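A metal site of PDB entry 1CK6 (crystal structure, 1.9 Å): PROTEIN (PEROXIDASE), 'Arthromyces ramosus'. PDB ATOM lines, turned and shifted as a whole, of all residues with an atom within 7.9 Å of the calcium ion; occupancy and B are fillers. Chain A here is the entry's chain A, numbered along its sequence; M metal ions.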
ATOM      1  N   PRO A 130      -8.896  -7.531  16.027  1.00  0.00           N
ATOM      2  CA  PRO A 130      -9.332  -6.529  16.994  1.00  0.00           C
ATOM      3  C   PRO A 130      -9.966  -7.122  18.249  1.00  0.00           C
ATOM      4  O   PRO A 130     -10.729  -8.100  18.169  1.00  0.00           O
ATOM      5  CB  PRO A 130     -10.300  -5.631  16.266  1.00  0.00           C
ATOM      6  CG  PRO A 130      -9.883  -5.830  14.809  1.00  0.00           C
ATOM      7  CD  PRO A 130      -9.470  -7.291  14.710  1.00  0.00           C
ATOM      8  N   ALA A 182     -13.545 -19.223  24.100  1.00  0.00           N
ATOM      9  CA  ALA A 182     -13.634 -17.855  23.581  1.00  0.00           C
ATOM     10  C   ALA A 182     -13.008 -17.845  22.178  1.00  0.00           C
ATOM     11  O   ALA A 182     -13.370 -16.998  21.351  1.00  0.00           O
ATOM     12  CB  ALA A 182     -12.849 -16.846  24.444  1.00  0.00           C
ATOM     13  N   ALA A 183     -12.101 -18.799  21.858  1.00  0.00           N
ATOM     14  CA  ALA A 183     -11.515 -18.864  20.544  1.00  0.00           C
ATOM     15  C   ALA A 183     -12.556 -19.149  19.457  1.00  0.00           C
ATOM     16  O   ALA A 183     -12.309 -18.812  18.298  1.00  0.00           O
ATOM     17  CB  ALA A 183     -10.465 -19.948  20.513  1.00  0.00           C
ATOM     18  N   HIS A 184     -13.765 -19.667  19.757  1.00  0.00           N
ATOM     19  CA  HIS A 184     -14.775 -19.834  18.737  1.00  0.00           C
ATOM     20  C   HIS A 184     -15.427 -18.484  18.361  1.00  0.00           C
ATOM     21  O   HIS A 184     -16.312 -18.413  17.496  1.00  0.00           O
ATOM     22  CB  HIS A 184     -15.828 -20.825  19.222  1.00  0.00           C
ATOM     23  CG  HIS A 184     -15.469 -22.295  19.069  1.00  0.00           C
ATOM     24  ND1 HIS A 184     -16.359 -23.330  19.260  1.00  0.00           N
ATOM     25  CD2 HIS A 184     -14.224 -22.786  18.678  1.00  0.00           C
ATOM     26  CE1 HIS A 184     -15.659 -24.446  18.992  1.00  0.00           C
ATOM     27  NE2 HIS A 184     -14.450 -24.163  18.651  1.00  0.00           N
ATOM     28  N   SER A 185     -15.008 -17.367  18.994  1.00  0.00           N
ATOM     29  CA  SER A 185     -15.429 -16.044  18.601  1.00  0.00           C
ATOM     30  C   SER A 185     -14.670 -15.648  17.323  1.00  0.00           C
ATOM     31  O   SER A 185     -14.998 -14.638  16.679  1.00  0.00           O
ATOM     32  CB  SER A 185     -15.108 -15.074  19.716  1.00  0.00           C
ATOM     33  OG  SER A 185     -15.539 -13.753  19.434  1.00  0.00           O
ATOM     34  N   LEU A 186     -13.646 -16.386  16.873  1.00  0.00           N
ATOM     35  CA  LEU A 186     -12.878 -16.075  15.665  1.00  0.00           C
ATOM     36  C   LEU A 186     -12.981 -17.402  14.902  1.00  0.00           C
ATOM     37  O   LEU A 186     -11.977 -18.067  14.642  1.00  0.00           O
ATOM     38  CB  LEU A 186     -11.440 -15.763  16.111  1.00  0.00           C
ATOM     39  CG  LEU A 186     -10.747 -14.379  16.253  1.00  0.00           C
ATOM     40  CD1 LEU A 186     -11.720 -13.239  16.263  1.00  0.00           C
ATOM     41  CD2 LEU A 186      -9.870 -14.449  17.501  1.00  0.00           C
ATOM     42  N   ALA A 187     -14.167 -17.863  14.524  1.00  0.00           N
ATOM     43  CA  ALA A 187     -14.262 -19.200  13.972  1.00  0.00           C
ATOM     44  C   ALA A 187     -15.289 -19.471  12.907  1.00  0.00           C
ATOM     45  O   ALA A 187     -16.324 -18.803  12.823  1.00  0.00           O
ATOM     46  CB  ALA A 187     -14.536 -20.154  15.120  1.00  0.00           C
ATOM     47  N   LEU A 201     -19.234 -19.032  13.354  1.00  0.00           N
ATOM     48  CA  LEU A 201     -19.796 -19.507  14.606  1.00  0.00           C
ATOM     49  C   LEU A 201     -20.338 -18.314  15.373  1.00  0.00           C
ATOM     50  O   LEU A 201     -21.055 -18.506  16.376  1.00  0.00           O
ATOM     51  CB  LEU A 201     -18.714 -20.284  15.374  1.00  0.00           C
ATOM     52  CG  LEU A 201     -18.696 -21.836  15.251  1.00  0.00           C
ATOM     53  CD1 LEU A 201     -18.786 -22.312  13.823  1.00  0.00           C
ATOM     54  CD2 LEU A 201     -17.420 -22.342  15.888  1.00  0.00           C
ATOM     55  N   ASP A 202     -20.000 -17.054  15.054  1.00  0.00           N
ATOM     56  CA  ASP A 202     -20.687 -15.936  15.655  1.00  0.00           C
ATOM     57  C   ASP A 202     -20.726 -14.878  14.573  1.00  0.00           C
ATOM     58  O   ASP A 202     -20.121 -15.075  13.505  1.00  0.00           O
ATOM     59  CB  ASP A 202     -19.990 -15.389  16.938  1.00  0.00           C
ATOM     60  CG  ASP A 202     -18.701 -14.571  16.953  1.00  0.00           C
ATOM     61  OD1 ASP A 202     -18.124 -14.244  15.913  1.00  0.00           O
ATOM     62  OD2 ASP A 202     -18.268 -14.243  18.048  1.00  0.00           O
ATOM     63  N   SER A 203     -21.405 -13.764  14.820  1.00  0.00           N
ATOM     64  CA  SER A 203     -21.534 -12.736  13.821  1.00  0.00           C
ATOM     65  C   SER A 203     -20.283 -11.901  13.564  1.00  0.00           C
ATOM     66  O   SER A 203     -20.281 -11.082  12.623  1.00  0.00           O
ATOM     67  CB  SER A 203     -22.702 -11.837  14.208  1.00  0.00           C
ATOM     68  OG  SER A 203     -22.517 -11.230  15.494  1.00  0.00           O
ATOM     69  N   THR A 204     -19.190 -12.005  14.350  1.00  0.00           N
ATOM     70  CA  THR A 204     -18.014 -11.217  14.114  1.00  0.00           C
ATOM     71  C   THR A 204     -16.811 -12.152  14.077  1.00  0.00           C
ATOM     72  O   THR A 204     -16.002 -12.118  15.004  1.00  0.00           O
ATOM     73  CB  THR A 204     -17.876 -10.198  15.231  1.00  0.00           C
ATOM     74  OG1 THR A 204     -17.962 -10.946  16.422  1.00  0.00           O
ATOM     75  CG2 THR A 204     -18.950  -9.127  15.250  1.00  0.00           C
ATOM     76  N   PRO A 205     -16.611 -12.988  13.035  1.00  0.00           N
ATOM     77  CA  PRO A 205     -15.503 -13.927  12.974  1.00  0.00           C
ATOM     78  C   PRO A 205     -14.146 -13.243  12.922  1.00  0.00           C
ATOM     79  O   PRO A 205     -13.112 -13.914  12.945  1.00  0.00           O
ATOM     80  CB  PRO A 205     -15.811 -14.803  11.750  1.00  0.00           C
ATOM     81  CG  PRO A 205     -16.515 -13.844  10.836  1.00  0.00           C
ATOM     82  CD  PRO A 205     -17.442 -13.136  11.841  1.00  0.00           C
ATOM     83  N   GLN A 206     -14.099 -11.912  12.786  1.00  0.00           N
ATOM     84  CA  GLN A 206     -12.830 -11.213  12.794  1.00  0.00           C
ATOM     85  C   GLN A 206     -12.698 -10.333  14.014  1.00  0.00           C
ATOM     86  O   GLN A 206     -11.785  -9.491  14.040  1.00  0.00           O
ATOM     87  CB  GLN A 206     -12.680 -10.377  11.526  1.00  0.00           C
ATOM     88  CG  GLN A 206     -12.597 -11.260  10.292  1.00  0.00           C
ATOM     89  CD  GLN A 206     -12.281 -10.423   9.080  1.00  0.00           C
ATOM     90  OE1 GLN A 206     -13.132  -9.675   8.608  1.00  0.00           O
ATOM     91  NE2 GLN A 206     -11.088 -10.435   8.498  1.00  0.00           N
ATOM     92  N   VAL A 207     -13.540 -10.412  15.048  1.00  0.00           N
ATOM     93  CA  VAL A 207     -13.366  -9.532  16.188  1.00  0.00           C
ATOM     94  C   VAL A 207     -13.385 -10.457  17.398  1.00  0.00           C
ATOM     95  O   VAL A 207     -14.310 -11.271  17.495  1.00  0.00           O
ATOM     96  CB  VAL A 207     -14.514  -8.508  16.319  1.00  0.00           C
ATOM     97  CG1 VAL A 207     -14.315  -7.693  17.582  1.00  0.00           C
ATOM     98  CG2 VAL A 207     -14.559  -7.589  15.117  1.00  0.00           C
ATOM     99  N   PHE A 208     -12.387 -10.413  18.280  1.00  0.00           N
ATOM    100  CA  PHE A 208     -12.348 -11.235  19.465  1.00  0.00           C
ATOM    101  C   PHE A 208     -13.224 -10.534  20.500  1.00  0.00           C
ATOM    102  O   PHE A 208     -12.825  -9.612  21.218  1.00  0.00           O
ATOM    103  CB  PHE A 208     -10.903 -11.371  19.964  1.00  0.00           C
ATOM    104  CG  PHE A 208     -10.764 -12.284  21.169  1.00  0.00           C
ATOM    105  CD1 PHE A 208     -10.930 -13.670  21.023  1.00  0.00           C
ATOM    106  CD2 PHE A 208     -10.483 -11.751  22.428  1.00  0.00           C
ATOM    107  CE1 PHE A 208     -10.812 -14.503  22.138  1.00  0.00           C
ATOM    108  CE2 PHE A 208     -10.364 -12.582  23.533  1.00  0.00           C
ATOM    109  CZ  PHE A 208     -10.529 -13.959  23.388  1.00  0.00           C
ATOM    110  N   ASP A 209     -14.452 -11.002  20.554  1.00  0.00           N
ATOM    111  CA  ASP A 209     -15.489 -10.477  21.430  1.00  0.00           C
ATOM    112  C   ASP A 209     -16.398 -11.555  22.048  1.00  0.00           C
ATOM    113  O   ASP A 209     -16.382 -12.752  21.770  1.00  0.00           O
ATOM    114  CB  ASP A 209     -16.349  -9.443  20.643  1.00  0.00           C
ATOM    115  CG  ASP A 209     -17.016 -10.032  19.385  1.00  0.00           C
ATOM    116  OD1 ASP A 209     -17.088 -11.253  19.223  1.00  0.00           O
ATOM    117  OD2 ASP A 209     -17.478  -9.252  18.546  1.00  0.00           O
ATOM    118  N   THR A 210     -17.300 -11.066  22.853  1.00  0.00           N
ATOM    119  CA  THR A 210     -18.317 -11.806  23.564  1.00  0.00           C
ATOM    120  C   THR A 210     -19.472 -12.372  22.688  1.00  0.00           C
ATOM    121  O   THR A 210     -20.250 -13.225  23.159  1.00  0.00           O
ATOM    122  CB  THR A 210     -18.563 -10.673  24.583  1.00  0.00           C
ATOM    123  OG1 THR A 210     -17.932 -11.009  25.809  1.00  0.00           O
ATOM    124  CG2 THR A 210     -19.939 -10.282  24.513  1.00  0.00           C
ATOM    125  N   GLN A 211     -19.625 -11.985  21.393  1.00  0.00           N
ATOM    126  CA  GLN A 211     -20.745 -12.420  20.556  1.00  0.00           C
ATOM    127  C   GLN A 211     -20.962 -13.920  20.504  1.00  0.00           C
ATOM    128  O   GLN A 211     -22.099 -14.356  20.534  1.00  0.00           O
ATOM    129  CB  GLN A 211     -20.607 -11.901  19.115  1.00  0.00           C
ATOM    130  CG  GLN A 211     -20.836 -10.401  18.962  1.00  0.00           C
ATOM    131  CD  GLN A 211     -22.084  -9.853  19.704  1.00  0.00           C
ATOM    132  OE1 GLN A 211     -21.993  -8.928  20.524  1.00  0.00           O
ATOM    133  NE2 GLN A 211     -23.283 -10.363  19.480  1.00  0.00           N
ATOM    134  N   PHE A 212     -19.925 -14.736  20.517  1.00  0.00           N
ATOM    135  CA  PHE A 212     -20.086 -16.181  20.484  1.00  0.00           C
ATOM    136  C   PHE A 212     -20.861 -16.680  21.708  1.00  0.00           C
ATOM    137  O   PHE A 212     -21.707 -17.542  21.549  1.00  0.00           O
ATOM    138  CB  PHE A 212     -18.692 -16.817  20.401  1.00  0.00           C
ATOM    139  CG  PHE A 212     -18.707 -18.307  20.719  1.00  0.00           C
ATOM    140  CD1 PHE A 212     -19.217 -19.212  19.788  1.00  0.00           C
ATOM    141  CD2 PHE A 212     -18.253 -18.727  21.979  1.00  0.00           C
ATOM    142  CE1 PHE A 212     -19.281 -20.569  20.143  1.00  0.00           C
ATOM    143  CE2 PHE A 212     -18.326 -20.080  22.324  1.00  0.00           C
ATOM    144  CZ  PHE A 212     -18.829 -21.000  21.411  1.00  0.00           C
ATOM    145  N   TYR A 213     -20.661 -16.136  22.895  1.00  0.00           N
ATOM    146  CA  TYR A 213     -21.372 -16.624  24.061  1.00  0.00           C
ATOM    147  C   TYR A 213     -22.849 -16.222  24.030  1.00  0.00           C
ATOM    148  O   TYR A 213     -23.752 -16.994  24.386  1.00  0.00           O
ATOM    149  CB  TYR A 213     -20.672 -16.105  25.310  1.00  0.00           C
ATOM    150  CG  TYR A 213     -19.287 -16.742  25.479  1.00  0.00           C
ATOM    151  CD1 TYR A 213     -19.156 -18.029  26.010  1.00  0.00           C
ATOM    152  CD2 TYR A 213     -18.133 -15.998  25.157  1.00  0.00           C
ATOM    153  CE1 TYR A 213     -17.885 -18.590  26.226  1.00  0.00           C
ATOM    154  CE2 TYR A 213     -16.863 -16.559  25.373  1.00  0.00           C
ATOM    155  CZ  TYR A 213     -16.751 -17.841  25.903  1.00  0.00           C
ATOM    156  OH  TYR A 213     -15.505 -18.341  26.177  1.00  0.00           O
ATOM    157  N   GLU A 215     -24.679 -15.498  21.226  1.00  0.00           N
ATOM    158  CA  GLU A 215     -25.338 -16.139  20.103  1.00  0.00           C
ATOM    159  C   GLU A 215     -25.570 -17.623  20.184  1.00  0.00           C
ATOM    160  O   GLU A 215     -26.572 -18.083  19.610  1.00  0.00           O
ATOM    161  CB  GLU A 215     -24.587 -15.775  18.851  1.00  0.00           C
ATOM    162  CG  GLU A 215     -24.791 -14.257  18.591  1.00  0.00           C
ATOM    163  CD  GLU A 215     -23.943 -13.678  17.481  1.00  0.00           C
ATOM    164  OE1 GLU A 215     -23.493 -14.393  16.603  1.00  0.00           O
ATOM    165  OE2 GLU A 215     -23.702 -12.479  17.485  1.00  0.00           O
ATOM    166  N   ASN A 266     -16.120  -7.906  27.380  1.00  0.00           N
ATOM    167  CA  ASN A 266     -15.006  -8.333  26.549  1.00  0.00           C
ATOM    168  C   ASN A 266     -13.735  -8.312  27.376  1.00  0.00           C
ATOM    169  O   ASN A 266     -12.858  -9.142  27.121  1.00  0.00           O
ATOM    170  CB  ASN A 266     -14.813  -7.415  25.364  1.00  0.00           C
ATOM    171  CG  ASN A 266     -15.907  -7.547  24.326  1.00  0.00           C
ATOM    172  OD1 ASN A 266     -16.220  -8.657  23.898  1.00  0.00           O
ATOM    173  ND2 ASN A 266     -16.516  -6.468  23.864  1.00  0.00           N
ATOM    174  N   MET A 269     -13.713 -11.512  29.570  1.00  0.00           N
ATOM    175  CA  MET A 269     -13.504 -12.630  28.662  1.00  0.00           C
ATOM    176  C   MET A 269     -12.019 -12.754  28.255  1.00  0.00           C
ATOM    177  O   MET A 269     -11.410 -13.827  28.374  1.00  0.00           O
ATOM    178  CB  MET A 269     -14.387 -12.465  27.416  1.00  0.00           C
ATOM    179  CG  MET A 269     -14.148 -13.588  26.418  1.00  0.00           C
ATOM    180  SD  MET A 269     -14.885 -13.293  24.790  1.00  0.00           S
ATOM    181  CE  MET A 269     -13.742 -12.071  24.198  1.00  0.00           C
ATOM    182  N   ASN A 303     -11.198  -3.218  20.402  1.00  0.00           N
ATOM    183  CA  ASN A 303     -12.536  -3.382  19.907  1.00  0.00           C
ATOM    184  C   ASN A 303     -13.318  -2.399  20.760  1.00  0.00           C
ATOM    185  O   ASN A 303     -13.276  -2.498  21.989  1.00  0.00           O
ATOM    186  CB  ASN A 303     -13.058  -4.752  20.165  1.00  0.00           C
ATOM    187  CG  ASN A 303     -14.550  -4.841  19.938  1.00  0.00           C
ATOM    188  OD1 ASN A 303     -15.105  -4.140  19.096  1.00  0.00           O
ATOM    189  ND2 ASN A 303     -15.256  -5.697  20.673  1.00  0.00           N
HETATM  190 CA    CA M   1     -16.418 -12.727  17.313  1.00  0.00          CA
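The calcium ion is bound by the backbone carbonyl oxygen (O) of Thr 204 (2.4 Å), the backbone carbonyl oxygen (O) of Ser 185 (2.5 Å), the side-chain carboxylate (OD2) of Asp 202 (2.5 Å), the side-chain carboxylate (OD1) of Asp 209 (2.5 Å), the side-chain hydroxyl (OG) of Ser 185 (2.5 Å), the side-chain hydroxyl (OG1) of Thr 204 (2.5 Å), the backbone carbonyl oxygen (O) of Val 207 (2.6 Å) and the side-chain carboxylate (OD1) of Asp 202 (2.7 Å).
Of the 24 residues printed, 5 come within 4 Å of the calcium ion.
Along chain A the residues within 4 Å of the calcium ion span positions 185 to 209.
The nearest printed residue that does not touch the calcium ion is Pro 205 (4.3 Å).
OD2 of Asp 202 lies close to N of Phe 212 (3.0 Å).
N of Gln 211 sits close to OD1 of Asp 209 (3.4 Å).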
